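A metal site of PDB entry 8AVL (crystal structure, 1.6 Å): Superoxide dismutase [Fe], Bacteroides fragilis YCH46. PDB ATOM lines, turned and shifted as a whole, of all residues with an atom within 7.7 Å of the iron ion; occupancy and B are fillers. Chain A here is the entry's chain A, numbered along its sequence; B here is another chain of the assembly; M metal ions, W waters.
Within 4 Å of the iron ion: His 26, His 74, Asp 158 and His 162. Along chain A the residues within 4 Å of the iron ion span positions 26 to 162.
OD1 of Asp 158 lies within hydrogen-bond range of N of Trp 160, 3.1 Å away. A ring nitrogen (ND1) of His 74 lies within hydrogen-bond range of the backbone carbonyl oxygen of Gln 70, at 2.6 Å. ND1 of His 162 sits close to ND1 of His 30 (3.5 Å). ND1 of His 162 lies within hydrogen-bond range of OE2 of Glu 161 of chain B (2.8 Å). The backbone carbonyl oxygen (O) of His 26 sits at hydrogen-bond distance from the backbone NH (N) of Leu 31, at 3.0 Å.
Water W1 lies within hydrogen-bond range of OD1 of Asp 158 (2.8 Å) and NE2 of Gln 70 (3.0 Å).
OD2 of Asp 158 is bound to the iron ion, 2.0 Å away. The iron ion is bound by a ring nitrogen (NE2) of His 74, 2.1 Å away. The iron ion is bound by water W1 (2.1 Å). A ring nitrogen (NE2) of His 162 is bound to the iron ion, at 2.2 Å. The iron ion is bound by a ring nitrogen (NE2) of His 26, at 2.2 Å. The iron ion has five donor atoms within binding distance.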
ATOM      1  N   HIS A  26     -36.675  16.462  -2.950  1.00  0.00           N
ATOM      2  CA  HIS A  26     -35.323  15.971  -3.190  1.00  0.00           C
ATOM      3  C   HIS A  26     -35.342  14.477  -3.516  1.00  0.00           C
ATOM      4  O   HIS A  26     -34.763  14.050  -4.527  1.00  0.00           O
ATOM      5  CB  HIS A  26     -34.455  16.292  -1.971  1.00  0.00           C
ATOM      6  CG  HIS A  26     -33.010  16.196  -2.245  1.00  0.00           C
ATOM      7  ND1 HIS A  26     -32.067  16.464  -1.282  1.00  0.00           N
ATOM      8  CD2 HIS A  26     -32.361  15.944  -3.368  1.00  0.00           C
ATOM      9  CE1 HIS A  26     -30.866  16.353  -1.806  1.00  0.00           C
ATOM     10  NE2 HIS A  26     -31.017  16.061  -3.109  1.00  0.00           N
ATOM     11  N   TYR A  27     -36.004  13.692  -2.646  1.00  0.00           N
ATOM     12  CA  TYR A  27     -36.196  12.271  -2.906  1.00  0.00           C
ATOM     13  C   TYR A  27     -37.306  12.025  -3.943  1.00  0.00           C
ATOM     14  O   TYR A  27     -37.101  11.346  -4.945  1.00  0.00           O
ATOM     15  CB  TYR A  27     -36.485  11.544  -1.588  1.00  0.00           C
ATOM     16  CG  TYR A  27     -36.825  10.076  -1.727  1.00  0.00           C
ATOM     17  CD1 TYR A  27     -35.825   9.107  -1.873  1.00  0.00           C
ATOM     18  CD2 TYR A  27     -38.138   9.664  -1.777  1.00  0.00           C
ATOM     19  CE1 TYR A  27     -36.129   7.768  -1.997  1.00  0.00           C
ATOM     20  CE2 TYR A  27     -38.467   8.319  -1.919  1.00  0.00           C
ATOM     21  CZ  TYR A  27     -37.461   7.362  -2.060  1.00  0.00           C
ATOM     22  OH  TYR A  27     -37.770   6.049  -2.200  1.00  0.00           O
ATOM     23  N   HIS A  30     -36.512  14.904  -7.450  1.00  0.00           N
ATOM     24  CA  HIS A  30     -35.183  14.909  -8.072  1.00  0.00           C
ATOM     25  C   HIS A  30     -34.680  13.483  -8.277  1.00  0.00           C
ATOM     26  O   HIS A  30     -34.307  13.132  -9.400  1.00  0.00           O
ATOM     27  CB  HIS A  30     -34.163  15.757  -7.297  1.00  0.00           C
ATOM     28  CG  HIS A  30     -34.437  17.232  -7.385  1.00  0.00           C
ATOM     29  ND1 HIS A  30     -33.948  18.077  -8.348  1.00  0.00           N
ATOM     30  CD2 HIS A  30     -35.218  18.013  -6.563  1.00  0.00           C
ATOM     31  CE1 HIS A  30     -34.407  19.303  -8.108  1.00  0.00           C
ATOM     32  NE2 HIS A  30     -35.170  19.297  -7.023  1.00  0.00           N
ATOM     33  N   LEU A  31     -34.660  12.655  -7.233  1.00  0.00           N
ATOM     34  CA  LEU A  31     -34.104  11.326  -7.388  1.00  0.00           C
ATOM     35  C   LEU A  31     -34.979  10.528  -8.345  1.00  0.00           C
ATOM     36  O   LEU A  31     -34.448   9.796  -9.189  1.00  0.00           O
ATOM     37  CB  LEU A  31     -33.918  10.612  -6.039  1.00  0.00           C
ATOM     38  CG  LEU A  31     -33.363   9.197  -6.095  1.00  0.00           C
ATOM     39  CD1 LEU A  31     -32.080   9.113  -6.888  1.00  0.00           C
ATOM     40  CD2 LEU A  31     -33.171   8.604  -4.683  1.00  0.00           C
ATOM     41  N   TYR A  34     -33.892  11.351 -11.835  1.00  0.00           N
ATOM     42  CA  TYR A  34     -32.608  10.744 -12.195  1.00  0.00           C
ATOM     43  C   TYR A  34     -32.783   9.258 -12.500  1.00  0.00           C
ATOM     44  O   TYR A  34     -32.182   8.773 -13.461  1.00  0.00           O
ATOM     45  CB  TYR A  34     -31.591  10.964 -11.070  1.00  0.00           C
ATOM     46  CG  TYR A  34     -31.189  12.408 -10.831  1.00  0.00           C
ATOM     47  CD1 TYR A  34     -30.748  13.220 -11.876  1.00  0.00           C
ATOM     48  CD2 TYR A  34     -31.173  12.935  -9.544  1.00  0.00           C
ATOM     49  CE1 TYR A  34     -30.338  14.523 -11.655  1.00  0.00           C
ATOM     50  CE2 TYR A  34     -30.742  14.241  -9.313  1.00  0.00           C
ATOM     51  CZ  TYR A  34     -30.314  15.030 -10.368  1.00  0.00           C
ATOM     52  OH  TYR A  34     -29.883  16.316 -10.094  1.00  0.00           O
ATOM     53  N   GLN A  70     -25.768  10.838 -10.172  1.00  0.00           N
ATOM     54  CA  GLN A  70     -26.759  11.410  -9.255  1.00  0.00           C
ATOM     55  C   GLN A  70     -27.615  10.346  -8.573  1.00  0.00           C
ATOM     56  O   GLN A  70     -27.933  10.474  -7.392  1.00  0.00           O
ATOM     57  CB  GLN A  70     -27.626  12.446  -9.932  1.00  0.00           C
ATOM     58  CG  GLN A  70     -26.925  13.776 -10.233  1.00  0.00           C
ATOM     59  CD  GLN A  70     -26.613  14.516  -8.952  1.00  0.00           C
ATOM     60  OE1 GLN A  70     -25.741  14.117  -8.186  1.00  0.00           O
ATOM     61  NE2 GLN A  70     -27.352  15.589  -8.683  1.00  0.00           N
ATOM     62  N   ASN A  73     -25.159   8.977  -5.897  1.00  0.00           N
ATOM     63  CA  ASN A  73     -24.934   9.968  -4.875  1.00  0.00           C
ATOM     64  C   ASN A  73     -26.134  10.049  -3.940  1.00  0.00           C
ATOM     65  O   ASN A  73     -25.993  10.036  -2.723  1.00  0.00           O
ATOM     66  CB  ASN A  73     -24.665  11.335  -5.467  1.00  0.00           C
ATOM     67  CG  ASN A  73     -23.260  11.564  -5.990  1.00  0.00           C
ATOM     68  OD1 ASN A  73     -22.287  11.090  -5.378  1.00  0.00           O
ATOM     69  ND2 ASN A  73     -23.135  12.328  -7.072  1.00  0.00           N
ATOM     70  N   HIS A  74     -27.338  10.173  -4.517  1.00  0.00           N
ATOM     71  CA  HIS A  74     -28.529  10.387  -3.700  1.00  0.00           C
ATOM     72  C   HIS A  74     -28.890   9.133  -2.896  1.00  0.00           C
ATOM     73  O   HIS A  74     -29.429   9.230  -1.798  1.00  0.00           O
ATOM     74  CB  HIS A  74     -29.746  10.809  -4.551  1.00  0.00           C
ATOM     75  CG  HIS A  74     -29.674  12.187  -5.041  1.00  0.00           C
ATOM     76  ND1 HIS A  74     -28.949  12.571  -6.151  1.00  0.00           N
ATOM     77  CD2 HIS A  74     -30.191  13.285  -4.521  1.00  0.00           C
ATOM     78  CE1 HIS A  74     -29.027  13.882  -6.298  1.00  0.00           C
ATOM     79  NE2 HIS A  74     -29.739  14.344  -5.276  1.00  0.00           N
ATOM     80  N   TYR A  77     -26.624   9.160  -0.031  1.00  0.00           N
ATOM     81  CA  TYR A  77     -27.024  10.292   0.799  1.00  0.00           C
ATOM     82  C   TYR A  77     -28.212   9.971   1.708  1.00  0.00           C
ATOM     83  O   TYR A  77     -28.121  10.126   2.928  1.00  0.00           O
ATOM     84  CB  TYR A  77     -27.324  11.473  -0.114  1.00  0.00           C
ATOM     85  CG  TYR A  77     -27.783  12.770   0.486  1.00  0.00           C
ATOM     86  CD1 TYR A  77     -26.871  13.635   1.095  1.00  0.00           C
ATOM     87  CD2 TYR A  77     -29.115  13.154   0.386  1.00  0.00           C
ATOM     88  CE1 TYR A  77     -27.279  14.876   1.572  1.00  0.00           C
ATOM     89  CE2 TYR A  77     -29.545  14.377   0.871  1.00  0.00           C
ATOM     90  CZ  TYR A  77     -28.611  15.260   1.434  1.00  0.00           C
ATOM     91  OH  TYR A  77     -29.005  16.530   1.830  1.00  0.00           O
ATOM     92  N   PHE A  78     -29.326   9.555   1.136  1.00  0.00           N
ATOM     93  CA  PHE A  78     -30.520   9.300   1.945  1.00  0.00           C
ATOM     94  C   PHE A  78     -30.293   8.153   2.938  1.00  0.00           C
ATOM     95  O   PHE A  78     -30.839   8.162   4.052  1.00  0.00           O
ATOM     96  CB  PHE A  78     -31.769   9.101   1.069  1.00  0.00           C
ATOM     97  CG  PHE A  78     -32.191  10.360   0.351  1.00  0.00           C
ATOM     98  CD1 PHE A  78     -32.537  11.503   1.076  1.00  0.00           C
ATOM     99  CD2 PHE A  78     -32.193  10.431  -1.058  1.00  0.00           C
ATOM    100  CE1 PHE A  78     -32.886  12.660   0.407  1.00  0.00           C
ATOM    101  CE2 PHE A  78     -32.552  11.603  -1.710  1.00  0.00           C
ATOM    102  CZ  PHE A  78     -32.893  12.710  -0.967  1.00  0.00           C
ATOM    103  N   GLY A 123     -22.583  20.306  -6.717  1.00  0.00           N
ATOM    104  CA  GLY A 123     -21.738  19.148  -6.547  1.00  0.00           C
ATOM    105  C   GLY A 123     -21.915  18.492  -5.192  1.00  0.00           C
ATOM    106  O   GLY A 123     -22.888  18.776  -4.488  1.00  0.00           O
ATOM    107  N   TRP A 124     -20.916  17.689  -4.825  1.00  0.00           N
ATOM    108  CA  TRP A 124     -20.905  16.856  -3.646  1.00  0.00           C
ATOM    109  C   TRP A 124     -19.534  16.958  -2.960  1.00  0.00           C
ATOM    110  O   TRP A 124     -18.505  16.816  -3.604  1.00  0.00           O
ATOM    111  CB  TRP A 124     -21.168  15.384  -4.017  1.00  0.00           C
ATOM    112  CG  TRP A 124     -22.552  15.157  -4.520  1.00  0.00           C
ATOM    113  CD1 TRP A 124     -23.060  15.471  -5.755  1.00  0.00           C
ATOM    114  CD2 TRP A 124     -23.650  14.628  -3.758  1.00  0.00           C
ATOM    115  NE1 TRP A 124     -24.390  15.163  -5.808  1.00  0.00           N
ATOM    116  CE2 TRP A 124     -24.772  14.621  -4.612  1.00  0.00           C
ATOM    117  CE3 TRP A 124     -23.771  14.061  -2.493  1.00  0.00           C
ATOM    118  CZ2 TRP A 124     -26.017  14.127  -4.209  1.00  0.00           C
ATOM    119  CZ3 TRP A 124     -25.012  13.602  -2.076  1.00  0.00           C
ATOM    120  CH2 TRP A 124     -26.100  13.618  -2.923  1.00  0.00           C
ATOM    121  N   ASP A 158     -24.547  16.675  -0.175  1.00  0.00           N
ATOM    122  CA  ASP A 158     -25.090  17.258  -1.381  1.00  0.00           C
ATOM    123  C   ASP A 158     -25.107  18.777  -1.225  1.00  0.00           C
ATOM    124  O   ASP A 158     -25.803  19.285  -0.340  1.00  0.00           O
ATOM    125  CB  ASP A 158     -26.523  16.782  -1.591  1.00  0.00           C
ATOM    126  CG  ASP A 158     -27.097  17.095  -2.943  1.00  0.00           C
ATOM    127  OD1 ASP A 158     -26.425  17.779  -3.767  1.00  0.00           O
ATOM    128  OD2 ASP A 158     -28.214  16.614  -3.191  1.00  0.00           O
ATOM    129  N   VAL A 159     -24.366  19.483  -2.080  1.00  0.00           N
ATOM    130  CA  VAL A 159     -24.379  20.946  -2.012  1.00  0.00           C
ATOM    131  C   VAL A 159     -24.976  21.571  -3.292  1.00  0.00           C
ATOM    132  O   VAL A 159     -24.908  22.774  -3.478  1.00  0.00           O
ATOM    133  CB  VAL A 159     -22.994  21.523  -1.630  1.00  0.00           C
ATOM    134  CG1 VAL A 159     -22.608  21.095  -0.251  1.00  0.00           C
ATOM    135  CG2 VAL A 159     -21.880  21.213  -2.606  1.00  0.00           C
ATOM    136  N   TRP A 160     -25.658  20.765  -4.121  1.00  0.00           N
ATOM    137  CA  TRP A 160     -26.665  21.318  -5.009  1.00  0.00           C
ATOM    138  C   TRP A 160     -27.670  22.125  -4.183  1.00  0.00           C
ATOM    139  O   TRP A 160     -28.094  21.706  -3.105  1.00  0.00           O
ATOM    140  CB  TRP A 160     -27.415  20.233  -5.802  1.00  0.00           C
ATOM    141  CG  TRP A 160     -26.634  19.485  -6.834  1.00  0.00           C
ATOM    142  CD1 TRP A 160     -25.508  18.736  -6.676  1.00  0.00           C
ATOM    143  CD2 TRP A 160     -27.000  19.380  -8.223  1.00  0.00           C
ATOM    144  NE1 TRP A 160     -25.137  18.178  -7.868  1.00  0.00           N
ATOM    145  CE2 TRP A 160     -26.030  18.560  -8.842  1.00  0.00           C
ATOM    146  CE3 TRP A 160     -28.033  19.924  -9.000  1.00  0.00           C
ATOM    147  CZ2 TRP A 160     -26.076  18.270 -10.209  1.00  0.00           C
ATOM    148  CZ3 TRP A 160     -28.059  19.646 -10.359  1.00  0.00           C
ATOM    149  CH2 TRP A 160     -27.109  18.794 -10.943  1.00  0.00           C
ATOM    150  N   GLU A 161     -28.070  23.276  -4.725  1.00  0.00           N
ATOM    151  CA  GLU A 161     -28.995  24.156  -4.003  1.00  0.00           C
ATOM    152  C   GLU A 161     -30.299  23.459  -3.627  1.00  0.00           C
ATOM    153  O   GLU A 161     -30.838  23.752  -2.570  1.00  0.00           O
ATOM    154  CB  GLU A 161     -29.207  25.456  -4.784  1.00  0.00           C
ATOM    155  CG  GLU A 161     -27.990  26.358  -4.696  1.00  0.00           C
ATOM    156  CD  GLU A 161     -28.048  27.640  -5.533  1.00  0.00           C
ATOM    157  OE1 GLU A 161     -28.511  27.598  -6.704  1.00  0.00           O
ATOM    158  OE2 GLU A 161     -27.585  28.671  -5.024  1.00  0.00           O
ATOM    159  N   HIS A 162     -30.802  22.534  -4.428  1.00  0.00           N
ATOM    160  CA  HIS A 162     -32.055  21.861  -4.109  1.00  0.00           C
ATOM    161  C   HIS A 162     -31.986  21.102  -2.777  1.00  0.00           C
ATOM    162  O   HIS A 162     -33.037  20.859  -2.177  1.00  0.00           O
ATOM    163  CB  HIS A 162     -32.566  20.968  -5.241  1.00  0.00           C
ATOM    164  CG  HIS A 162     -31.697  19.811  -5.582  1.00  0.00           C
ATOM    165  ND1 HIS A 162     -31.212  19.646  -6.849  1.00  0.00           N
ATOM    166  CD2 HIS A 162     -31.243  18.776  -4.884  1.00  0.00           C
ATOM    167  CE1 HIS A 162     -30.470  18.565  -6.891  1.00  0.00           C
ATOM    168  NE2 HIS A 162     -30.487  17.999  -5.726  1.00  0.00           N
ATOM    169  N   ALA A 163     -30.783  20.739  -2.311  1.00  0.00           N
ATOM    170  CA  ALA A 163     -30.634  19.983  -1.076  1.00  0.00           C
ATOM    171  C   ALA A 163     -31.021  20.812   0.155  1.00  0.00           C
ATOM    172  O   ALA A 163     -31.360  20.235   1.190  1.00  0.00           O
ATOM    173  CB  ALA A 163     -29.209  19.472  -0.907  1.00  0.00           C
ATOM    174  N   TYR A 164     -30.940  22.159   0.035  1.00  0.00           N
ATOM    175  CA  TYR A 164     -31.078  23.026   1.189  1.00  0.00           C
ATOM    176  C   TYR A 164     -31.889  24.292   0.927  1.00  0.00           C
ATOM    177  O   TYR A 164     -32.268  24.944   1.897  1.00  0.00           O
ATOM    178  CB  TYR A 164     -29.702  23.393   1.749  1.00  0.00           C
ATOM    179  CG  TYR A 164     -28.744  24.100   0.799  1.00  0.00           C
ATOM    180  CD1 TYR A 164     -28.780  25.470   0.606  1.00  0.00           C
ATOM    181  CD2 TYR A 164     -27.784  23.381   0.097  1.00  0.00           C
ATOM    182  CE1 TYR A 164     -27.868  26.116  -0.231  1.00  0.00           C
ATOM    183  CE2 TYR A 164     -26.866  24.010  -0.726  1.00  0.00           C
ATOM    184  CZ  TYR A 164     -26.906  25.383  -0.906  1.00  0.00           C
ATOM    185  OH  TYR A 164     -26.016  25.992  -1.729  1.00  0.00           O
ATOM    186  N   GLU B 161     -30.240  26.846  -9.533  1.00  0.00           N
ATOM    187  CA  GLU B 161     -31.493  26.560  -8.839  1.00  0.00           C
ATOM    188  C   GLU B 161     -32.020  27.749  -8.034  1.00  0.00           C
ATOM    189  O   GLU B 161     -33.228  27.945  -7.983  1.00  0.00           O
ATOM    190  CB  GLU B 161     -31.374  25.281  -8.021  1.00  0.00           C
ATOM    191  CG  GLU B 161     -31.277  24.044  -8.907  1.00  0.00           C
ATOM    192  CD  GLU B 161     -31.097  22.718  -8.221  1.00  0.00           C
ATOM    193  OE1 GLU B 161     -30.260  22.659  -7.245  1.00  0.00           O
ATOM    194  OE2 GLU B 161     -31.819  21.742  -8.622  1.00  0.00           O
HETATM  195 FE    FE M   1     -29.499  16.380  -4.675  1.00  0.00          FE
HETATM  196  O   HOH W   1     -27.815  16.723  -5.962  1.00  0.00           O
